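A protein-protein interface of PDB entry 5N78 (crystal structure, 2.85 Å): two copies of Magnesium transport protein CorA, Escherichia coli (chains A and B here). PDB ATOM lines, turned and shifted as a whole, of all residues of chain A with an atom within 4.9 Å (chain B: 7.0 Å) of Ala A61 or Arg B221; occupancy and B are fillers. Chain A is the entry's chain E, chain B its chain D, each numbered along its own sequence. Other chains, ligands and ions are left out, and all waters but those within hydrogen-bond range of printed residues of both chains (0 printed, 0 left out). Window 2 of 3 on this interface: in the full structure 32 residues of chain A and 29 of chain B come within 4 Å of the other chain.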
ATOM      1  N   ILE A  59      -8.630  -1.759 -29.527  1.00  0.00           N
ATOM      2  CA  ILE A  59      -8.565  -0.318 -29.362  1.00  0.00           C
ATOM      3  C   ILE A  59      -9.350   0.210 -28.187  1.00  0.00           C
ATOM      4  O   ILE A  59      -9.216   1.357 -27.805  1.00  0.00           O
ATOM      5  CB  ILE A  59      -9.039   0.397 -30.645  1.00  0.00           C
ATOM      6  CG1 ILE A  59     -10.437  -0.042 -31.065  1.00  0.00           C
ATOM      7  CG2 ILE A  59      -8.081   0.145 -31.790  1.00  0.00           C
ATOM      8  CD1 ILE A  59     -11.095   0.987 -31.959  1.00  0.00           C
ATOM      9  N   GLU A  60     -10.252  -0.611 -27.704  1.00  0.00           N
ATOM     10  CA  GLU A  60     -11.038  -0.388 -26.509  1.00  0.00           C
ATOM     11  C   GLU A  60     -10.149  -0.045 -25.318  1.00  0.00           C
ATOM     12  O   GLU A  60      -9.144  -0.678 -25.105  1.00  0.00           O
ATOM     13  CB  GLU A  60     -11.857  -1.702 -26.263  1.00  0.00           C
ATOM     14  CG  GLU A  60     -11.676  -2.858 -27.259  1.00  0.00           C
ATOM     15  CD  GLU A  60     -11.859  -4.230 -26.647  1.00  0.00           C
ATOM     16  OE1 GLU A  60     -12.477  -4.248 -25.560  1.00  0.00           O
ATOM     17  OE2 GLU A  60     -11.440  -5.292 -27.233  1.00  0.00           O
ATOM     18  N   ALA A  61     -10.525   0.960 -24.529  1.00  0.00           N
ATOM     19  CA  ALA A  61      -9.759   1.343 -23.309  1.00  0.00           C
ATOM     20  C   ALA A  61      -9.410   0.165 -22.413  1.00  0.00           C
ATOM     21  O   ALA A  61      -8.260   0.022 -21.999  1.00  0.00           O
ATOM     22  CB  ALA A  61     -10.527   2.373 -22.476  1.00  0.00           C
ATOM     23  N   SER A  62     -10.395  -0.666 -22.107  1.00  0.00           N
ATOM     24  CA  SER A  62     -10.161  -1.787 -21.212  1.00  0.00           C
ATOM     25  C   SER A  62      -9.180  -2.807 -21.765  1.00  0.00           C
ATOM     26  O   SER A  62      -8.652  -3.611 -21.032  1.00  0.00           O
ATOM     27  CB  SER A  62     -11.461  -2.485 -20.901  1.00  0.00           C
ATOM     28  OG  SER A  62     -11.988  -3.081 -22.075  1.00  0.00           O
ATOM     29  N   ALA A  63      -8.923  -2.776 -23.067  1.00  0.00           N
ATOM     30  CA  ALA A  63      -7.981  -3.700 -23.689  1.00  0.00           C
ATOM     31  C   ALA A  63      -6.592  -3.135 -23.742  1.00  0.00           C
ATOM     32  O   ALA A  63      -5.660  -3.870 -23.980  1.00  0.00           O
ATOM     33  CB  ALA A  63      -8.445  -4.034 -25.092  1.00  0.00           C
ATOM     34  N   ARG A  64      -6.475  -1.821 -23.570  1.00  0.00           N
ATOM     35  CA  ARG A  64      -5.214  -1.088 -23.694  1.00  0.00           C
ATOM     36  C   ARG A  64      -4.619  -0.585 -22.379  1.00  0.00           C
ATOM     37  O   ARG A  64      -3.406  -0.539 -22.247  1.00  0.00           O
ATOM     38  CB  ARG A  64      -5.425   0.178 -24.508  1.00  0.00           C
ATOM     39  CG  ARG A  64      -5.915  -0.011 -25.907  1.00  0.00           C
ATOM     40  CD  ARG A  64      -5.440   1.106 -26.805  1.00  0.00           C
ATOM     41  NE  ARG A  64      -4.897   0.470 -27.990  1.00  0.00           N
ATOM     42  CZ  ARG A  64      -3.911   0.961 -28.717  1.00  0.00           C
ATOM     43  NH1 ARG A  64      -3.345   2.116 -28.407  1.00  0.00           N
ATOM     44  NH2 ARG A  64      -3.499   0.294 -29.780  1.00  0.00           N
ATOM     45  N   PHE A  65      -5.459  -0.118 -21.447  1.00  0.00           N
ATOM     46  CA  PHE A  65      -4.992   0.462 -20.176  1.00  0.00           C
ATOM     47  C   PHE A  65      -5.650  -0.311 -19.032  1.00  0.00           C
ATOM     48  O   PHE A  65      -6.836  -0.119 -18.751  1.00  0.00           O
ATOM     49  CB  PHE A  65      -5.328   1.955 -20.109  1.00  0.00           C
ATOM     50  CG  PHE A  65      -5.113   2.670 -21.405  1.00  0.00           C
ATOM     51  CD1 PHE A  65      -3.846   2.751 -21.968  1.00  0.00           C
ATOM     52  CD2 PHE A  65      -6.169   3.239 -22.087  1.00  0.00           C
ATOM     53  CE1 PHE A  65      -3.650   3.374 -23.202  1.00  0.00           C
ATOM     54  CE2 PHE A  65      -5.984   3.882 -23.301  1.00  0.00           C
ATOM     55  CZ  PHE A  65      -4.725   3.942 -23.863  1.00  0.00           C
ATOM     56  N   LEU B 213     -21.365  -2.939 -10.470  1.00  0.00           N
ATOM     57  CA  LEU B 213     -21.192  -1.506 -10.658  1.00  0.00           C
ATOM     58  C   LEU B 213     -19.866  -1.215 -11.323  1.00  0.00           C
ATOM     59  O   LEU B 213     -19.814  -0.472 -12.287  1.00  0.00           O
ATOM     60  CB  LEU B 213     -21.289  -0.769  -9.336  1.00  0.00           C
ATOM     61  CG  LEU B 213     -21.522   0.721  -9.493  1.00  0.00           C
ATOM     62  CD1 LEU B 213     -22.860   0.993 -10.152  1.00  0.00           C
ATOM     63  CD2 LEU B 213     -21.455   1.372  -8.129  1.00  0.00           C
ATOM     64  N   GLU B 214     -18.795  -1.830 -10.835  1.00  0.00           N
ATOM     65  CA  GLU B 214     -17.496  -1.635 -11.468  1.00  0.00           C
ATOM     66  C   GLU B 214     -17.542  -2.089 -12.936  1.00  0.00           C
ATOM     67  O   GLU B 214     -16.993  -1.430 -13.813  1.00  0.00           O
ATOM     68  CB  GLU B 214     -16.385  -2.357 -10.689  1.00  0.00           C
ATOM     69  CG  GLU B 214     -14.962  -2.153 -11.234  1.00  0.00           C
ATOM     70  CD  GLU B 214     -14.668  -0.713 -11.676  1.00  0.00           C
ATOM     71  OE1 GLU B 214     -14.818   0.222 -10.849  1.00  0.00           O
ATOM     72  OE2 GLU B 214     -14.295  -0.505 -12.862  1.00  0.00           O
ATOM     73  N   GLN B 215     -18.213  -3.207 -13.191  1.00  0.00           N
ATOM     74  CA  GLN B 215     -18.335  -3.784 -14.541  1.00  0.00           C
ATOM     75  C   GLN B 215     -19.001  -2.823 -15.496  1.00  0.00           C
ATOM     76  O   GLN B 215     -18.504  -2.591 -16.586  1.00  0.00           O
ATOM     77  CB  GLN B 215     -19.164  -5.044 -14.457  1.00  0.00           C
ATOM     78  CG  GLN B 215     -19.111  -5.952 -15.657  1.00  0.00           C
ATOM     79  CD  GLN B 215     -19.887  -7.236 -15.415  1.00  0.00           C
ATOM     80  OE1 GLN B 215     -20.295  -7.532 -14.284  1.00  0.00           O
ATOM     81  NE2 GLN B 215     -20.156  -7.970 -16.492  1.00  0.00           N
ATOM     82  N   ALA B 216     -20.109  -2.244 -15.053  1.00  0.00           N
ATOM     83  CA  ALA B 216     -20.798  -1.210 -15.801  1.00  0.00           C
ATOM     84  C   ALA B 216     -19.901  -0.011 -16.052  1.00  0.00           C
ATOM     85  O   ALA B 216     -19.857   0.504 -17.169  1.00  0.00           O
ATOM     86  CB  ALA B 216     -22.065  -0.780 -15.086  1.00  0.00           C
ATOM     87  N   ARG B 217     -19.188   0.450 -15.034  1.00  0.00           N
ATOM     88  CA  ARG B 217     -18.285   1.573 -15.224  1.00  0.00           C
ATOM     89  C   ARG B 217     -17.189   1.256 -16.229  1.00  0.00           C
ATOM     90  O   ARG B 217     -16.869   2.086 -17.047  1.00  0.00           O
ATOM     91  CB  ARG B 217     -17.673   2.006 -13.911  1.00  0.00           C
ATOM     92  CG  ARG B 217     -18.675   2.638 -12.961  1.00  0.00           C
ATOM     93  CD  ARG B 217     -17.980   3.581 -11.980  1.00  0.00           C
ATOM     94  NE  ARG B 217     -18.929   4.262 -11.101  1.00  0.00           N
ATOM     95  CZ  ARG B 217     -19.171   3.945  -9.827  1.00  0.00           C
ATOM     96  NH1 ARG B 217     -18.531   2.942  -9.230  1.00  0.00           N
ATOM     97  NH2 ARG B 217     -20.067   4.652  -9.141  1.00  0.00           N
ATOM     98  N   GLU B 218     -16.628   0.056 -16.178  1.00  0.00           N
ATOM     99  CA  GLU B 218     -15.639  -0.369 -17.169  1.00  0.00           C
ATOM    100  C   GLU B 218     -16.190  -0.273 -18.599  1.00  0.00           C
ATOM    101  O   GLU B 218     -15.523   0.234 -19.513  1.00  0.00           O
ATOM    102  CB  GLU B 218     -15.150  -1.791 -16.870  1.00  0.00           C
ATOM    103  CG  GLU B 218     -14.480  -2.521 -18.041  1.00  0.00           C
ATOM    104  CD  GLU B 218     -13.245  -3.315 -17.620  1.00  0.00           C
ATOM    105  OE1 GLU B 218     -12.241  -2.685 -17.201  1.00  0.00           O
ATOM    106  OE2 GLU B 218     -13.261  -4.566 -17.710  1.00  0.00           O
ATOM    107  N   ILE B 219     -17.418  -0.731 -18.783  1.00  0.00           N
ATOM    108  CA  ILE B 219     -18.062  -0.656 -20.084  1.00  0.00           C
ATOM    109  C   ILE B 219     -18.268   0.785 -20.503  1.00  0.00           C
ATOM    110  O   ILE B 219     -18.024   1.115 -21.637  1.00  0.00           O
ATOM    111  CB  ILE B 219     -19.424  -1.379 -20.113  1.00  0.00           C
ATOM    112  CG1 ILE B 219     -19.260  -2.855 -19.752  1.00  0.00           C
ATOM    113  CG2 ILE B 219     -20.031  -1.287 -21.504  1.00  0.00           C
ATOM    114  CD1 ILE B 219     -20.537  -3.657 -19.797  1.00  0.00           C
ATOM    115  N   LEU B 220     -18.726   1.645 -19.602  1.00  0.00           N
ATOM    116  CA  LEU B 220     -18.882   3.058 -19.940  1.00  0.00           C
ATOM    117  C   LEU B 220     -17.572   3.665 -20.360  1.00  0.00           C
ATOM    118  O   LEU B 220     -17.541   4.491 -21.247  1.00  0.00           O
ATOM    119  CB  LEU B 220     -19.464   3.847 -18.770  1.00  0.00           C
ATOM    120  CG  LEU B 220     -20.986   3.750 -18.666  1.00  0.00           C
ATOM    121  CD1 LEU B 220     -21.480   4.194 -17.306  1.00  0.00           C
ATOM    122  CD2 LEU B 220     -21.683   4.589 -19.731  1.00  0.00           C
ATOM    123  N   ARG B 221     -16.490   3.270 -19.703  1.00  0.00           N
ATOM    124  CA  ARG B 221     -15.165   3.802 -19.986  1.00  0.00           C
ATOM    125  C   ARG B 221     -14.737   3.396 -21.385  1.00  0.00           C
ATOM    126  O   ARG B 221     -14.023   4.133 -22.051  1.00  0.00           O
ATOM    127  CB  ARG B 221     -14.156   3.256 -18.980  1.00  0.00           C
ATOM    128  CG  ARG B 221     -13.236   4.293 -18.360  1.00  0.00           C
ATOM    129  CD  ARG B 221     -12.419   3.702 -17.188  1.00  0.00           C
ATOM    130  NE  ARG B 221     -13.187   3.501 -15.941  1.00  0.00           N
ATOM    131  CZ  ARG B 221     -13.378   2.334 -15.303  1.00  0.00           C
ATOM    132  NH1 ARG B 221     -12.868   1.183 -15.749  1.00  0.00           N
ATOM    133  NH2 ARG B 221     -14.100   2.311 -14.191  1.00  0.00           N
ATOM    134  N   ASP B 222     -15.151   2.211 -21.817  1.00  0.00           N
ATOM    135  CA  ASP B 222     -14.816   1.730 -23.159  1.00  0.00           C
ATOM    136  C   ASP B 222     -15.562   2.488 -24.222  1.00  0.00           C
ATOM    137  O   ASP B 222     -14.983   2.857 -25.238  1.00  0.00           O
ATOM    138  CB  ASP B 222     -15.139   0.247 -23.318  1.00  0.00           C
ATOM    139  CG  ASP B 222     -14.063  -0.678 -22.716  1.00  0.00           C
ATOM    140  OD1 ASP B 222     -12.952  -0.188 -22.365  1.00  0.00           O
ATOM    141  OD2 ASP B 222     -14.336  -1.906 -22.612  1.00  0.00           O
ATOM    142  N   ILE B 223     -16.844   2.740 -23.987  1.00  0.00           N
ATOM    143  CA  ILE B 223     -17.623   3.555 -24.893  1.00  0.00           C
ATOM    144  C   ILE B 223     -17.034   4.953 -25.008  1.00  0.00           C
ATOM    145  O   ILE B 223     -16.872   5.459 -26.110  1.00  0.00           O
ATOM    146  CB  ILE B 223     -19.067   3.664 -24.454  1.00  0.00           C
ATOM    147  CG1 ILE B 223     -19.718   2.293 -24.527  1.00  0.00           C
ATOM    148  CG2 ILE B 223     -19.828   4.585 -25.376  1.00  0.00           C
ATOM    149  CD1 ILE B 223     -21.132   2.255 -23.986  1.00  0.00           C
ATOM    150  N   GLU B 224     -16.688   5.572 -23.887  1.00  0.00           N
ATOM    151  CA  GLU B 224     -16.073   6.886 -23.932  1.00  0.00           C
ATOM    152  C   GLU B 224     -14.832   6.828 -24.808  1.00  0.00           C
ATOM    153  O   GLU B 224     -14.492   7.808 -25.449  1.00  0.00           O
ATOM    154  CB  GLU B 224     -15.726   7.358 -22.531  1.00  0.00           C
ATOM    155  CG  GLU B 224     -15.151   8.763 -22.392  1.00  0.00           C
ATOM    156  CD  GLU B 224     -14.385   8.976 -21.052  1.00  0.00           C
ATOM    157  OE1 GLU B 224     -14.457   8.130 -20.097  1.00  0.00           O
ATOM    158  OE2 GLU B 224     -13.677  10.013 -20.939  1.00  0.00           O
ATOM    159  N   SER B 225     -14.159   5.682 -24.861  1.00  0.00           N
ATOM    160  CA  SER B 225     -12.943   5.566 -25.656  1.00  0.00           C
ATOM    161  C   SER B 225     -13.144   5.186 -27.108  1.00  0.00           C
ATOM    162  O   SER B 225     -12.211   5.318 -27.884  1.00  0.00           O
ATOM    163  CB  SER B 225     -11.987   4.553 -25.047  1.00  0.00           C
ATOM    164  OG  SER B 225     -12.359   3.242 -25.392  1.00  0.00           O
ATOM    165  N   LEU B 226     -14.322   4.687 -27.472  1.00  0.00           N
ATOM    166  CA  LEU B 226     -14.593   4.324 -28.867  1.00  0.00           C
ATOM    167  C   LEU B 226     -15.262   5.427 -29.647  1.00  0.00           C
ATOM    168  O   LEU B 226     -15.038   5.548 -30.836  1.00  0.00           O
ATOM    169  CB  LEU B 226     -15.464   3.074 -28.949  1.00  0.00           C
ATOM    170  CG  LEU B 226     -14.809   1.790 -28.433  1.00  0.00           C
ATOM    171  CD1 LEU B 226     -15.805   0.658 -28.435  1.00  0.00           C
ATOM    172  CD2 LEU B 226     -13.613   1.392 -29.271  1.00  0.00           C
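OD1 of Asp B222 lies within hydrogen-bond range of N of Ala A61 (3.4 Å).
The side-chain carboxylate (OD1) of Asp B222 is in hydrogen-bond range of the backbone NH (N) of Ser A62, at 2.6 Å.
The backbone NH of Ala A61 lies within hydrogen-bond range of the side-chain hydroxyl of Ser B225 (3.1 Å).
The side-chain carboxylate (OE2) of Glu B214 is in salt-bridge range of the guanidinium group (NH2) of Arg B221 (3.1 Å).
O of Asp B222 is in hydrogen-bond range of OG of Ser B225 (2.7 Å).
Among the printed residues, merely in contact across the chains: Ile A59 with Leu B226 (3.7 Å), Glu A60 with Ser B225 (3.96 Å), Ala A61 with Arg B221 (3.9 Å) and Ser A62 with Glu B218 (3.8 Å).
Printed residues of chain B within 4 Å of Glu A60: Ser B225 (3.96 Å).
Of chain B, only Arg B221 (3.9 Å), Asp B222 (3.4 Å) and Ser B225 (3.1 Å) come within 4 Å of Ala A61.
Of the printed residues of chain B, Ser A62 touches Glu B218 (3.8 Å) and Asp B222 (2.6 Å).
Of the printed residues of chain A, Glu B218 touches Ser A62 (3.8 Å).
Printed residues of chain A within 4 Å of Arg B221: Ala A61.
Printed residues of chain A within 4 Å of Asp B222: Ala A61 and Ser A62.
Printed residues of chain A within 4 Å of Leu B226: Ile A59 (3.7 Å).
The nearest residue of chain B that does not touch Ala A61 is Leu B226 (5.7 Å).
The nearest printed residue of chain A that does not touch Leu B226 is Glu A60 (4.2 Å).
Of the 14 printed residues of chain B, 5 touch a printed residue of chain A.
No position is printed for both chains.
Of the 7 pairs that touch across the chains among the printed residues, none has its exchanged pair printed and touching as well.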
